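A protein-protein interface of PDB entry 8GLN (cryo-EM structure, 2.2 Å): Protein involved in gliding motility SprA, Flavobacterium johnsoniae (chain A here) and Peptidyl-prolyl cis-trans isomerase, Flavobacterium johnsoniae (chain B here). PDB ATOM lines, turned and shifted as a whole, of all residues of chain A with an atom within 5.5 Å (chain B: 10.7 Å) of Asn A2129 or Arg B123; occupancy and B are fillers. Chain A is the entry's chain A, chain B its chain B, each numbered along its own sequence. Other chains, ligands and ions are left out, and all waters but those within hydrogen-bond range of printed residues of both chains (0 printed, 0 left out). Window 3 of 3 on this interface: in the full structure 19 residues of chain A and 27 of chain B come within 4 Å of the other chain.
Among the printed residues, 7 pairs touch across the chains.
Among the printed residues, no Asp or Glu carboxylate lies within 4 Å of a Lys or Arg side-chain nitrogen of the other chain.
Among the printed residues, pairs that only touch across the chains: Asn A2129 with Arg B123 and Gln A2228 with Arg B123.
The side-chain amide oxygen of Gln A395 lies close to the side-chain amide oxygen of Asn B96 (2.8 Å).
The side-chain hydroxyl (OG) of Ser B121 lies within hydrogen-bond range of the side-chain amide nitrogen (NE2) of Gln A395 (2.8 Å).
The side-chain amide nitrogen (ND2) of Asn B94 lies within hydrogen-bond range of the side-chain carboxylate (OD2) of Asp A2127.
The backbone carbonyl oxygen (O) of Thr B124 is in hydrogen-bond range of the backbone NH (N) of Gln A2228.
The side-chain amino group (NZ) of Lys B130 sits at hydrogen-bond distance from the side-chain amide oxygen (OE1) of Gln A2228, 2.8 Å away.
No residue of chain B comes within 4 Å of Pro A2123.
No residue of chain B comes within 4 Å of Pro A2128.
Asn A2129 touches just one residue of chain B: Arg B123.
No residue of chain B comes within 4 Å of Ala A2131.
Val A2132 touches none of the printed residues of chain B.
No residue of chain B comes within 4 Å of Tyr A2133.
Of chain B, only Arg B123, Thr B124 and Lys B130 come within 4 Å of Gln A2228.
Of the printed residues of chain A, Asn B94 touches Asp A2127 (2.7 Å).
Of the printed residues of chain A, Ser B121 touches Gln A395.
Of chain A, only Asn A2129 and Gln A2228 come within 4 Å of Arg B123.
The nearest residue of chain A that does not touch Arg B123 is Pro A2128 (4.4 Å).
The nearest printed residue of chain A that does not touch Asn B96 is Pro A2128 (10.9 Å).
The side-chain amide nitrogen of Gln A2228 lies within hydrogen-bond range of the backbone carbonyl oxygen of Thr A2232.
OG1 of Thr B92 lies within hydrogen-bond range of O of Asn B94 (3.5 Å).
The guanidinium group (NH1) of Arg B123 lies within hydrogen-bond range of the side-chain amide oxygen (OD1) of Asn B94 (2.6 Å).
The side-chain hydroxyl of Ser B119 lies within hydrogen-bond range of the side-chain amide nitrogen of Asn B96 (3.4 Å).
The backbone carbonyl oxygen (O) of Tyr B120 sits close to the side-chain amide oxygen (OD1) of Asn B96, 3.1 Å away.
The backbone NH (N) of Asn B176 lies within hydrogen-bond range of the backbone carbonyl oxygen (O) of Asn B96, 3.3 Å away.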
ATOM      1  N   GLN A 395      18.828  -2.974 -31.925  1.00  0.00           N
ATOM      2  CA  GLN A 395      18.237  -1.635 -31.922  1.00  0.00           C
ATOM      3  C   GLN A 395      17.743  -1.227 -33.307  1.00  0.00           C
ATOM      4  O   GLN A 395      16.536  -1.105 -33.537  1.00  0.00           O
ATOM      5  CB  GLN A 395      19.256  -0.621 -31.392  1.00  0.00           C
ATOM      6  CG  GLN A 395      19.100  -0.289 -29.922  1.00  0.00           C
ATOM      7  CD  GLN A 395      20.278   0.493 -29.386  1.00  0.00           C
ATOM      8  OE1 GLN A 395      21.088   1.014 -30.149  1.00  0.00           O
ATOM      9  NE2 GLN A 395      20.380   0.580 -28.065  1.00  0.00           N
ATOM     10  N   PRO A2123       5.179  -1.903 -22.260  1.00  0.00           N
ATOM     11  CA  PRO A2123       5.234  -1.871 -23.727  1.00  0.00           C
ATOM     12  C   PRO A2123       4.643  -3.119 -24.361  1.00  0.00           C
ATOM     13  O   PRO A2123       4.128  -3.999 -23.665  1.00  0.00           O
ATOM     14  CB  PRO A2123       6.732  -1.745 -24.032  1.00  0.00           C
ATOM     15  CG  PRO A2123       7.449  -2.097 -22.779  1.00  0.00           C
ATOM     16  CD  PRO A2123       6.492  -2.137 -21.634  1.00  0.00           C
ATOM     17  N   ASP A2127       8.676  -5.357 -27.573  1.00  0.00           N
ATOM     18  CA  ASP A2127       9.660  -4.466 -26.979  1.00  0.00           C
ATOM     19  C   ASP A2127      10.583  -5.246 -26.045  1.00  0.00           C
ATOM     20  O   ASP A2127      10.129  -6.144 -25.326  1.00  0.00           O
ATOM     21  CB  ASP A2127       8.958  -3.337 -26.221  1.00  0.00           C
ATOM     22  CG  ASP A2127       9.926  -2.307 -25.660  1.00  0.00           C
ATOM     23  OD1 ASP A2127      10.679  -2.633 -24.718  1.00  0.00           O
ATOM     24  OD2 ASP A2127       9.932  -1.167 -26.166  1.00  0.00           O
ATOM     25  N   PRO A2128      11.885  -4.938 -26.036  1.00  0.00           N
ATOM     26  CA  PRO A2128      12.806  -5.654 -25.136  1.00  0.00           C
ATOM     27  C   PRO A2128      12.512  -5.454 -23.658  1.00  0.00           C
ATOM     28  O   PRO A2128      12.888  -6.316 -22.854  1.00  0.00           O
ATOM     29  CB  PRO A2128      14.183  -5.083 -25.507  1.00  0.00           C
ATOM     30  CG  PRO A2128      13.903  -3.819 -26.259  1.00  0.00           C
ATOM     31  CD  PRO A2128      12.587  -4.008 -26.935  1.00  0.00           C
ATOM     32  N   ASN A2129      11.861  -4.359 -23.272  1.00  0.00           N
ATOM     33  CA  ASN A2129      11.630  -4.042 -21.868  1.00  0.00           C
ATOM     34  C   ASN A2129      10.226  -4.400 -21.398  1.00  0.00           C
ATOM     35  O   ASN A2129       9.810  -3.945 -20.328  1.00  0.00           O
ATOM     36  CB  ASN A2129      11.903  -2.557 -21.614  1.00  0.00           C
ATOM     37  CG  ASN A2129      13.374  -2.264 -21.391  1.00  0.00           C
ATOM     38  OD1 ASN A2129      14.169  -3.171 -21.147  1.00  0.00           O
ATOM     39  ND2 ASN A2129      13.742  -0.992 -21.475  1.00  0.00           N
ATOM     40  N   TYR A2130       9.486  -5.195 -22.173  1.00  0.00           N
ATOM     41  CA  TYR A2130       8.157  -5.623 -21.744  1.00  0.00           C
ATOM     42  C   TYR A2130       8.230  -6.437 -20.458  1.00  0.00           C
ATOM     43  O   TYR A2130       7.476  -6.191 -19.507  1.00  0.00           O
ATOM     44  CB  TYR A2130       7.489  -6.434 -22.856  1.00  0.00           C
ATOM     45  CG  TYR A2130       6.323  -7.273 -22.387  1.00  0.00           C
ATOM     46  CD1 TYR A2130       5.068  -6.710 -22.196  1.00  0.00           C
ATOM     47  CD2 TYR A2130       6.474  -8.631 -22.135  1.00  0.00           C
ATOM     48  CE1 TYR A2130       4.001  -7.473 -21.768  1.00  0.00           C
ATOM     49  CE2 TYR A2130       5.415  -9.400 -21.704  1.00  0.00           C
ATOM     50  CZ  TYR A2130       4.179  -8.817 -21.524  1.00  0.00           C
ATOM     51  OH  TYR A2130       3.120  -9.583 -21.096  1.00  0.00           O
ATOM     52  N   ALA A2131       9.140  -7.413 -20.411  1.00  0.00           N
ATOM     53  CA  ALA A2131       9.242  -8.278 -19.241  1.00  0.00           C
ATOM     54  C   ALA A2131       9.704  -7.506 -18.013  1.00  0.00           C
ATOM     55  O   ALA A2131       9.202  -7.735 -16.908  1.00  0.00           O
ATOM     56  CB  ALA A2131      10.189  -9.442 -19.530  1.00  0.00           C
ATOM     57  N   VAL A2132      10.667  -6.598 -18.183  1.00  0.00           N
ATOM     58  CA  VAL A2132      11.157  -5.816 -17.051  1.00  0.00           C
ATOM     59  C   VAL A2132      10.047  -4.935 -16.492  1.00  0.00           C
ATOM     60  O   VAL A2132       9.869  -4.834 -15.272  1.00  0.00           O
ATOM     61  CB  VAL A2132      12.389  -4.990 -17.467  1.00  0.00           C
ATOM     62  CG1 VAL A2132      12.646  -3.866 -16.472  1.00  0.00           C
ATOM     63  CG2 VAL A2132      13.609  -5.887 -17.591  1.00  0.00           C
ATOM     64  N   TYR A2133       9.281  -4.289 -17.373  1.00  0.00           N
ATOM     65  CA  TYR A2133       8.178  -3.449 -16.917  1.00  0.00           C
ATOM     66  C   TYR A2133       7.101  -4.275 -16.227  1.00  0.00           C
ATOM     67  O   TYR A2133       6.533  -3.846 -15.216  1.00  0.00           O
ATOM     68  CB  TYR A2133       7.589  -2.672 -18.095  1.00  0.00           C
ATOM     69  CG  TYR A2133       8.278  -1.354 -18.361  1.00  0.00           C
ATOM     70  CD1 TYR A2133       9.651  -1.294 -18.554  1.00  0.00           C
ATOM     71  CD2 TYR A2133       7.557  -0.169 -18.416  1.00  0.00           C
ATOM     72  CE1 TYR A2133      10.286  -0.093 -18.797  1.00  0.00           C
ATOM     73  CE2 TYR A2133       8.184   1.037 -18.659  1.00  0.00           C
ATOM     74  CZ  TYR A2133       9.548   1.069 -18.846  1.00  0.00           C
ATOM     75  OH  TYR A2133      10.178   2.267 -19.088  1.00  0.00           O
ATOM     76  N   THR A2134       6.804  -5.463 -16.759  1.00  0.00           N
ATOM     77  CA  THR A2134       5.784  -6.310 -16.149  1.00  0.00           C
ATOM     78  C   THR A2134       6.232  -6.834 -14.788  1.00  0.00           C
ATOM     79  O   THR A2134       5.415  -6.968 -13.870  1.00  0.00           O
ATOM     80  CB  THR A2134       5.439  -7.473 -17.080  1.00  0.00           C
ATOM     81  OG1 THR A2134       5.236  -6.977 -18.409  1.00  0.00           O
ATOM     82  CG2 THR A2134       4.175  -8.173 -16.612  1.00  0.00           C
ATOM     83  N   GLN A2228      20.464   5.515 -16.539  1.00  0.00           N
ATOM     84  CA  GLN A2228      19.835   4.217 -16.341  1.00  0.00           C
ATOM     85  C   GLN A2228      20.628   3.136 -17.062  1.00  0.00           C
ATOM     86  O   GLN A2228      21.151   3.362 -18.157  1.00  0.00           O
ATOM     87  CB  GLN A2228      18.386   4.226 -16.836  1.00  0.00           C
ATOM     88  CG  GLN A2228      17.394   4.756 -15.814  1.00  0.00           C
ATOM     89  CD  GLN A2228      15.971   4.768 -16.332  1.00  0.00           C
ATOM     90  OE1 GLN A2228      15.594   5.631 -17.124  1.00  0.00           O
ATOM     91  NE2 GLN A2228      15.170   3.810 -15.885  1.00  0.00           N
ATOM     92  N   VAL A2230      21.039  -1.142 -18.354  1.00  0.00           N
ATOM     93  CA  VAL A2230      20.287  -1.989 -19.274  1.00  0.00           C
ATOM     94  C   VAL A2230      19.017  -2.537 -18.634  1.00  0.00           C
ATOM     95  O   VAL A2230      18.062  -2.873 -19.341  1.00  0.00           O
ATOM     96  CB  VAL A2230      21.197  -3.124 -19.797  1.00  0.00           C
ATOM     97  CG1 VAL A2230      21.560  -4.090 -18.678  1.00  0.00           C
ATOM     98  CG2 VAL A2230      20.546  -3.850 -20.966  1.00  0.00           C
ATOM     99  N   THR A2232      17.136  -0.732 -16.621  1.00  0.00           N
ATOM    100  CA  THR A2232      16.442   0.503 -16.259  1.00  0.00           C
ATOM    101  C   THR A2232      16.713   0.937 -14.823  1.00  0.00           C
ATOM    102  O   THR A2232      16.057   1.861 -14.331  1.00  0.00           O
ATOM    103  CB  THR A2232      14.925   0.416 -16.488  1.00  0.00           C
ATOM    104  OG1 THR A2232      14.347  -0.534 -15.584  1.00  0.00           O
ATOM    105  CG2 THR A2232      14.621  -0.002 -17.917  1.00  0.00           C
ATOM    106  N   PRO B  91      12.925  10.899 -33.068  1.00  0.00           N
ATOM    107  CA  PRO B  91      13.336   9.741 -32.268  1.00  0.00           C
ATOM    108  C   PRO B  91      12.220   9.285 -31.343  1.00  0.00           C
ATOM    109  O   PRO B  91      11.455  10.094 -30.813  1.00  0.00           O
ATOM    110  CB  PRO B  91      14.547  10.251 -31.475  1.00  0.00           C
ATOM    111  CG  PRO B  91      14.550  11.729 -31.611  1.00  0.00           C
ATOM    112  CD  PRO B  91      13.539  12.159 -32.620  1.00  0.00           C
ATOM    113  N   THR B  92      12.134   7.973 -31.154  1.00  0.00           N
ATOM    114  CA  THR B  92      11.163   7.373 -30.257  1.00  0.00           C
ATOM    115  C   THR B  92      11.864   6.906 -28.985  1.00  0.00           C
ATOM    116  O   THR B  92      13.063   7.117 -28.790  1.00  0.00           O
ATOM    117  CB  THR B  92      10.437   6.216 -30.946  1.00  0.00           C
ATOM    118  OG1 THR B  92      11.334   5.110 -31.099  1.00  0.00           O
ATOM    119  CG2 THR B  92       9.933   6.648 -32.315  1.00  0.00           C
ATOM    120  N   LEU B  93      11.097   6.259 -28.103  1.00  0.00           N
ATOM    121  CA  LEU B  93      11.670   5.765 -26.855  1.00  0.00           C
ATOM    122  C   LEU B  93      12.753   4.727 -27.118  1.00  0.00           C
ATOM    123  O   LEU B  93      13.811   4.746 -26.478  1.00  0.00           O
ATOM    124  CB  LEU B  93      10.572   5.184 -25.966  1.00  0.00           C
ATOM    125  CG  LEU B  93      10.338   5.894 -24.631  1.00  0.00           C
ATOM    126  CD1 LEU B  93       9.551   5.005 -23.680  1.00  0.00           C
ATOM    127  CD2 LEU B  93      11.658   6.324 -24.003  1.00  0.00           C
ATOM    128  N   ASN B  94      12.509   3.812 -28.056  1.00  0.00           N
ATOM    129  CA  ASN B  94      13.505   2.820 -28.456  1.00  0.00           C
ATOM    130  C   ASN B  94      14.166   3.306 -29.743  1.00  0.00           C
ATOM    131  O   ASN B  94      13.923   2.795 -30.836  1.00  0.00           O
ATOM    132  CB  ASN B  94      12.859   1.449 -28.629  1.00  0.00           C
ATOM    133  CG  ASN B  94      12.212   0.945 -27.355  1.00  0.00           C
ATOM    134  OD1 ASN B  94      12.889   0.450 -26.455  1.00  0.00           O
ATOM    135  ND2 ASN B  94      10.893   1.071 -27.273  1.00  0.00           N
ATOM    136  N   SER B  95      15.021   4.315 -29.599  1.00  0.00           N
ATOM    137  CA  SER B  95      15.728   4.885 -30.736  1.00  0.00           C
ATOM    138  C   SER B  95      17.128   5.287 -30.305  1.00  0.00           C
ATOM    139  O   SER B  95      17.314   5.855 -29.227  1.00  0.00           O
ATOM    140  CB  SER B  95      14.984   6.098 -31.308  1.00  0.00           C
ATOM    141  OG  SER B  95      14.147   5.722 -32.387  1.00  0.00           O
ATOM    142  N   ASN B  96      18.107   5.000 -31.157  1.00  0.00           N
ATOM    143  CA  ASN B  96      19.487   5.383 -30.905  1.00  0.00           C
ATOM    144  C   ASN B  96      19.757   6.742 -31.535  1.00  0.00           C
ATOM    145  O   ASN B  96      19.439   6.964 -32.708  1.00  0.00           O
ATOM    146  CB  ASN B  96      20.450   4.334 -31.463  1.00  0.00           C
ATOM    147  CG  ASN B  96      21.735   4.240 -30.666  1.00  0.00           C
ATOM    148  OD1 ASN B  96      21.752   3.717 -29.553  1.00  0.00           O
ATOM    149  ND2 ASN B  96      22.821   4.748 -31.234  1.00  0.00           N
ATOM    150  N   ILE B  97      20.337   7.650 -30.754  1.00  0.00           N
ATOM    151  CA  ILE B  97      20.597   9.012 -31.195  1.00  0.00           C
ATOM    152  C   ILE B  97      22.064   9.340 -30.967  1.00  0.00           C
ATOM    153  O   ILE B  97      22.719   8.763 -30.094  1.00  0.00           O
ATOM    154  CB  ILE B  97      19.698  10.037 -30.465  1.00  0.00           C
ATOM    155  CG1 ILE B  97      19.983  10.021 -28.962  1.00  0.00           C
ATOM    156  CG2 ILE B  97      18.230   9.755 -30.737  1.00  0.00           C
ATOM    157  CD1 ILE B  97      19.448  11.224 -28.223  1.00  0.00           C
ATOM    158  N   SER B 119      26.775   8.467 -29.042  1.00  0.00           N
ATOM    159  CA  SER B 119      25.557   7.710 -29.289  1.00  0.00           C
ATOM    160  C   SER B 119      24.891   7.301 -27.980  1.00  0.00           C
ATOM    161  O   SER B 119      25.549   6.812 -27.058  1.00  0.00           O
ATOM    162  CB  SER B 119      25.858   6.469 -30.131  1.00  0.00           C
ATOM    163  OG  SER B 119      25.609   6.716 -31.503  1.00  0.00           O
ATOM    164  N   TYR B 120      23.576   7.503 -27.911  1.00  0.00           N
ATOM    165  CA  TYR B 120      22.788   7.160 -26.736  1.00  0.00           C
ATOM    166  C   TYR B 120      21.530   6.421 -27.171  1.00  0.00           C
ATOM    167  O   TYR B 120      21.112   6.496 -28.328  1.00  0.00           O
ATOM    168  CB  TYR B 120      22.408   8.404 -25.922  1.00  0.00           C
ATOM    169  CG  TYR B 120      23.556   9.021 -25.160  1.00  0.00           C
ATOM    170  CD1 TYR B 120      24.412   8.239 -24.396  1.00  0.00           C
ATOM    171  CD2 TYR B 120      23.781  10.390 -25.199  1.00  0.00           C
ATOM    172  CE1 TYR B 120      25.460   8.803 -23.698  1.00  0.00           C
ATOM    173  CE2 TYR B 120      24.825  10.963 -24.503  1.00  0.00           C
ATOM    174  CZ  TYR B 120      25.661  10.165 -23.754  1.00  0.00           C
ATOM    175  OH  TYR B 120      26.703  10.735 -23.062  1.00  0.00           O
ATOM    176  N   SER B 121      20.926   5.705 -26.223  1.00  0.00           N
ATOM    177  CA  SER B 121      19.716   4.936 -26.483  1.00  0.00           C
ATOM    178  C   SER B 121      18.433   5.719 -26.231  1.00  0.00           C
ATOM    179  O   SER B 121      17.354   5.231 -26.587  1.00  0.00           O
ATOM    180  CB  SER B 121      19.705   3.664 -25.628  1.00  0.00           C
ATOM    181  OG  SER B 121      20.478   2.643 -26.232  1.00  0.00           O
ATOM    182  N   LEU B 122      18.520   6.879 -25.580  1.00  0.00           N
ATOM    183  CA  LEU B 122      17.413   7.815 -25.391  1.00  0.00           C
ATOM    184  C   LEU B 122      16.388   7.284 -24.392  1.00  0.00           C
ATOM    185  O   LEU B 122      15.481   8.013 -23.982  1.00  0.00           O
ATOM    186  CB  LEU B 122      16.745   8.146 -26.733  1.00  0.00           C
ATOM    187  CG  LEU B 122      15.910   9.427 -26.863  1.00  0.00           C
ATOM    188  CD1 LEU B 122      14.422   9.155 -26.693  1.00  0.00           C
ATOM    189  CD2 LEU B 122      16.378  10.495 -25.881  1.00  0.00           C
ATOM    190  N   ARG B 123      16.537   6.032 -23.966  1.00  0.00           N
ATOM    191  CA  ARG B 123      15.727   5.489 -22.886  1.00  0.00           C
ATOM    192  C   ARG B 123      16.526   5.289 -21.609  1.00  0.00           C
ATOM    193  O   ARG B 123      15.940   4.969 -20.569  1.00  0.00           O
ATOM    194  CB  ARG B 123      15.080   4.163 -23.308  1.00  0.00           C
ATOM    195  CG  ARG B 123      15.957   2.938 -23.118  1.00  0.00           C
ATOM    196  CD  ARG B 123      15.208   1.670 -23.489  1.00  0.00           C
ATOM    197  NE  ARG B 123      16.106   0.593 -23.886  1.00  0.00           N
ATOM    198  CZ  ARG B 123      16.215   0.127 -25.123  1.00  0.00           C
ATOM    199  NH1 ARG B 123      15.491   0.621 -26.114  1.00  0.00           N
ATOM    200  NH2 ARG B 123      17.071  -0.859 -25.373  1.00  0.00           N
ATOM    201  N   THR B 124      17.843   5.467 -21.668  1.00  0.00           N
ATOM    202  CA  THR B 124      18.715   5.402 -20.507  1.00  0.00           C
ATOM    203  C   THR B 124      19.101   6.780 -19.988  1.00  0.00           C
ATOM    204  O   THR B 124      19.877   6.874 -19.034  1.00  0.00           O
ATOM    205  CB  THR B 124      19.980   4.609 -20.847  1.00  0.00           C
ATOM    206  OG1 THR B 124      20.861   5.424 -21.628  1.00  0.00           O
ATOM    207  CG2 THR B 124      19.625   3.364 -21.640  1.00  0.00           C
ATOM    208  N   LEU B 125      18.579   7.845 -20.588  1.00  0.00           N
ATOM    209  CA  LEU B 125      18.953   9.208 -20.252  1.00  0.00           C
ATOM    210  C   LEU B 125      17.992   9.787 -19.216  1.00  0.00           C
ATOM    211  O   LEU B 125      17.012   9.157 -18.811  1.00  0.00           O
ATOM    212  CB  LEU B 125      18.991  10.073 -21.514  1.00  0.00           C
ATOM    213  CG  LEU B 125      19.682   9.462 -22.735  1.00  0.00           C
ATOM    214  CD1 LEU B 125      19.579  10.393 -23.931  1.00  0.00           C
ATOM    215  CD2 LEU B 125      21.135   9.137 -22.433  1.00  0.00           C
ATOM    216  N   ILE B 126      18.285  11.008 -18.782  1.00  0.00           N
ATOM    217  CA  ILE B 126      17.463  11.711 -17.800  1.00  0.00           C
ATOM    218  C   ILE B 126      16.113  12.040 -18.429  1.00  0.00           C
ATOM    219  O   ILE B 126      16.023  12.180 -19.657  1.00  0.00           O
ATOM    220  CB  ILE B 126      18.170  12.976 -17.286  1.00  0.00           C
ATOM    221  CG1 ILE B 126      18.614  13.859 -18.453  1.00  0.00           C
ATOM    222  CG2 ILE B 126      19.358  12.607 -16.417  1.00  0.00           C
ATOM    223  CD1 ILE B 126      19.105  15.223 -18.026  1.00  0.00           C
ATOM    224  N   PRO B 127      15.043  12.157 -17.635  1.00  0.00           N
ATOM    225  CA  PRO B 127      13.716  12.408 -18.221  1.00  0.00           C
ATOM    226  C   PRO B 127      13.641  13.665 -19.068  1.00  0.00           C
ATOM    227  O   PRO B 127      12.879  13.695 -20.044  1.00  0.00           O
ATOM    228  CB  PRO B 127      12.810  12.508 -16.987  1.00  0.00           C
ATOM    229  CG  PRO B 127      13.487  11.671 -15.965  1.00  0.00           C
ATOM    230  CD  PRO B 127      14.962  11.853 -16.195  1.00  0.00           C
ATOM    231  N   GLY B 128      14.399  14.708 -18.721  1.00  0.00           N
ATOM    232  CA  GLY B 128      14.373  15.924 -19.519  1.00  0.00           C
ATOM    233  C   GLY B 128      14.747  15.672 -20.966  1.00  0.00           C
ATOM    234  O   GLY B 128      14.098  16.173 -21.886  1.00  0.00           O
ATOM    235  N   TRP B 129      15.797  14.880 -21.186  1.00  0.00           N
ATOM    236  CA  TRP B 129      16.152  14.488 -22.544  1.00  0.00           C
ATOM    237  C   TRP B 129      15.063  13.629 -23.175  1.00  0.00           C
ATOM    238  O   TRP B 129      14.736  13.805 -24.353  1.00  0.00           O
ATOM    239  CB  TRP B 129      17.487  13.749 -22.547  1.00  0.00           C
ATOM    240  CG  TRP B 129      18.667  14.646 -22.382  1.00  0.00           C
ATOM    241  CD1 TRP B 129      18.811  15.660 -21.482  1.00  0.00           C
ATOM    242  CD2 TRP B 129      19.879  14.610 -23.142  1.00  0.00           C
ATOM    243  NE1 TRP B 129      20.038  16.257 -21.634  1.00  0.00           N
ATOM    244  CE2 TRP B 129      20.712  15.630 -22.647  1.00  0.00           C
ATOM    245  CE3 TRP B 129      20.339  13.813 -24.193  1.00  0.00           C
ATOM    246  CZ2 TRP B 129      21.980  15.873 -23.167  1.00  0.00           C
ATOM    247  CZ3 TRP B 129      21.596  14.055 -24.706  1.00  0.00           C
ATOM    248  CH2 TRP B 129      22.401  15.075 -24.195  1.00  0.00           C
ATOM    249  N   LYS B 130      14.484  12.705 -22.402  1.00  0.00           N
ATOM    250  CA  LYS B 130      13.429  11.847 -22.932  1.00  0.00           C
ATOM    251  C   LYS B 130      12.238  12.656 -23.429  1.00  0.00           C
ATOM    252  O   LYS B 130      11.535  12.222 -24.347  1.00  0.00           O
ATOM    253  CB  LYS B 130      12.974  10.849 -21.868  1.00  0.00           C
ATOM    254  CG  LYS B 130      13.968   9.745 -21.568  1.00  0.00           C
ATOM    255  CD  LYS B 130      13.414   8.800 -20.519  1.00  0.00           C
ATOM    256  CE  LYS B 130      14.449   7.780 -20.088  1.00  0.00           C
ATOM    257  NZ  LYS B 130      13.930   6.882 -19.022  1.00  0.00           N
ATOM    258  N   GLU B 131      11.990  13.822 -22.834  1.00  0.00           N
ATOM    259  CA  GLU B 131      10.918  14.691 -23.303  1.00  0.00           C
ATOM    260  C   GLU B 131      11.362  15.672 -24.380  1.00  0.00           C
ATOM    261  O   GLU B 131      10.540  16.057 -25.220  1.00  0.00           O
ATOM    262  CB  GLU B 131      10.311  15.473 -22.135  1.00  0.00           C
ATOM    263  CG  GLU B 131      10.065  14.644 -20.890  1.00  0.00           C
ATOM    264  CD  GLU B 131       9.179  15.351 -19.888  1.00  0.00           C
ATOM    265  OE1 GLU B 131       8.549  16.362 -20.262  1.00  0.00           O
ATOM    266  OE2 GLU B 131       9.112  14.899 -18.726  1.00  0.00           O
ATOM    267  N   ILE B 133      14.315  15.490 -26.661  1.00  0.00           N
ATOM    268  CA  ILE B 133      14.888  14.988 -27.915  1.00  0.00           C
ATOM    269  C   ILE B 133      13.822  14.621 -28.938  1.00  0.00           C
ATOM    270  O   ILE B 133      13.984  14.979 -30.114  1.00  0.00           O
ATOM    271  CB  ILE B 133      15.870  13.845 -27.625  1.00  0.00           C
ATOM    272  CG1 ILE B 133      16.944  14.303 -26.634  1.00  0.00           C
ATOM    273  CG2 ILE B 133      16.490  13.331 -28.916  1.00  0.00           C
ATOM    274  CD1 ILE B 133      18.183  14.884 -27.282  1.00  0.00           C
ATOM    275  N   PRO B 134      12.733  13.919 -28.596  1.00  0.00           N
ATOM    276  CA  PRO B 134      11.719  13.603 -29.620  1.00  0.00           C
ATOM    277  C   PRO B 134      11.088  14.820 -30.286  1.00  0.00           C
ATOM    278  O   PRO B 134      10.319  14.643 -31.239  1.00  0.00           O
ATOM    279  CB  PRO B 134      10.659  12.803 -28.851  1.00  0.00           C
ATOM    280  CG  PRO B 134      11.302  12.338 -27.621  1.00  0.00           C
ATOM    281  CD  PRO B 134      12.538  13.131 -27.363  1.00  0.00           C
ATOM    282  N   ASN B 176      20.096   7.221 -35.940  1.00  0.00           N
ATOM    283  CA  ASN B 176      20.422   5.860 -36.352  1.00  0.00           C
ATOM    284  C   ASN B 176      20.146   4.847 -35.243  1.00  0.00           C
ATOM    285  O   ASN B 176      19.084   4.225 -35.207  1.00  0.00           O
ATOM    286  CB  ASN B 176      21.885   5.773 -36.791  1.00  0.00           C
ATOM    287  CG  ASN B 176      22.852   6.247 -35.719  1.00  0.00           C
ATOM    288  OD1 ASN B 176      22.455   6.556 -34.594  1.00  0.00           O
ATOM    289  ND2 ASN B 176      24.132   6.307 -36.065  1.00  0.00           N
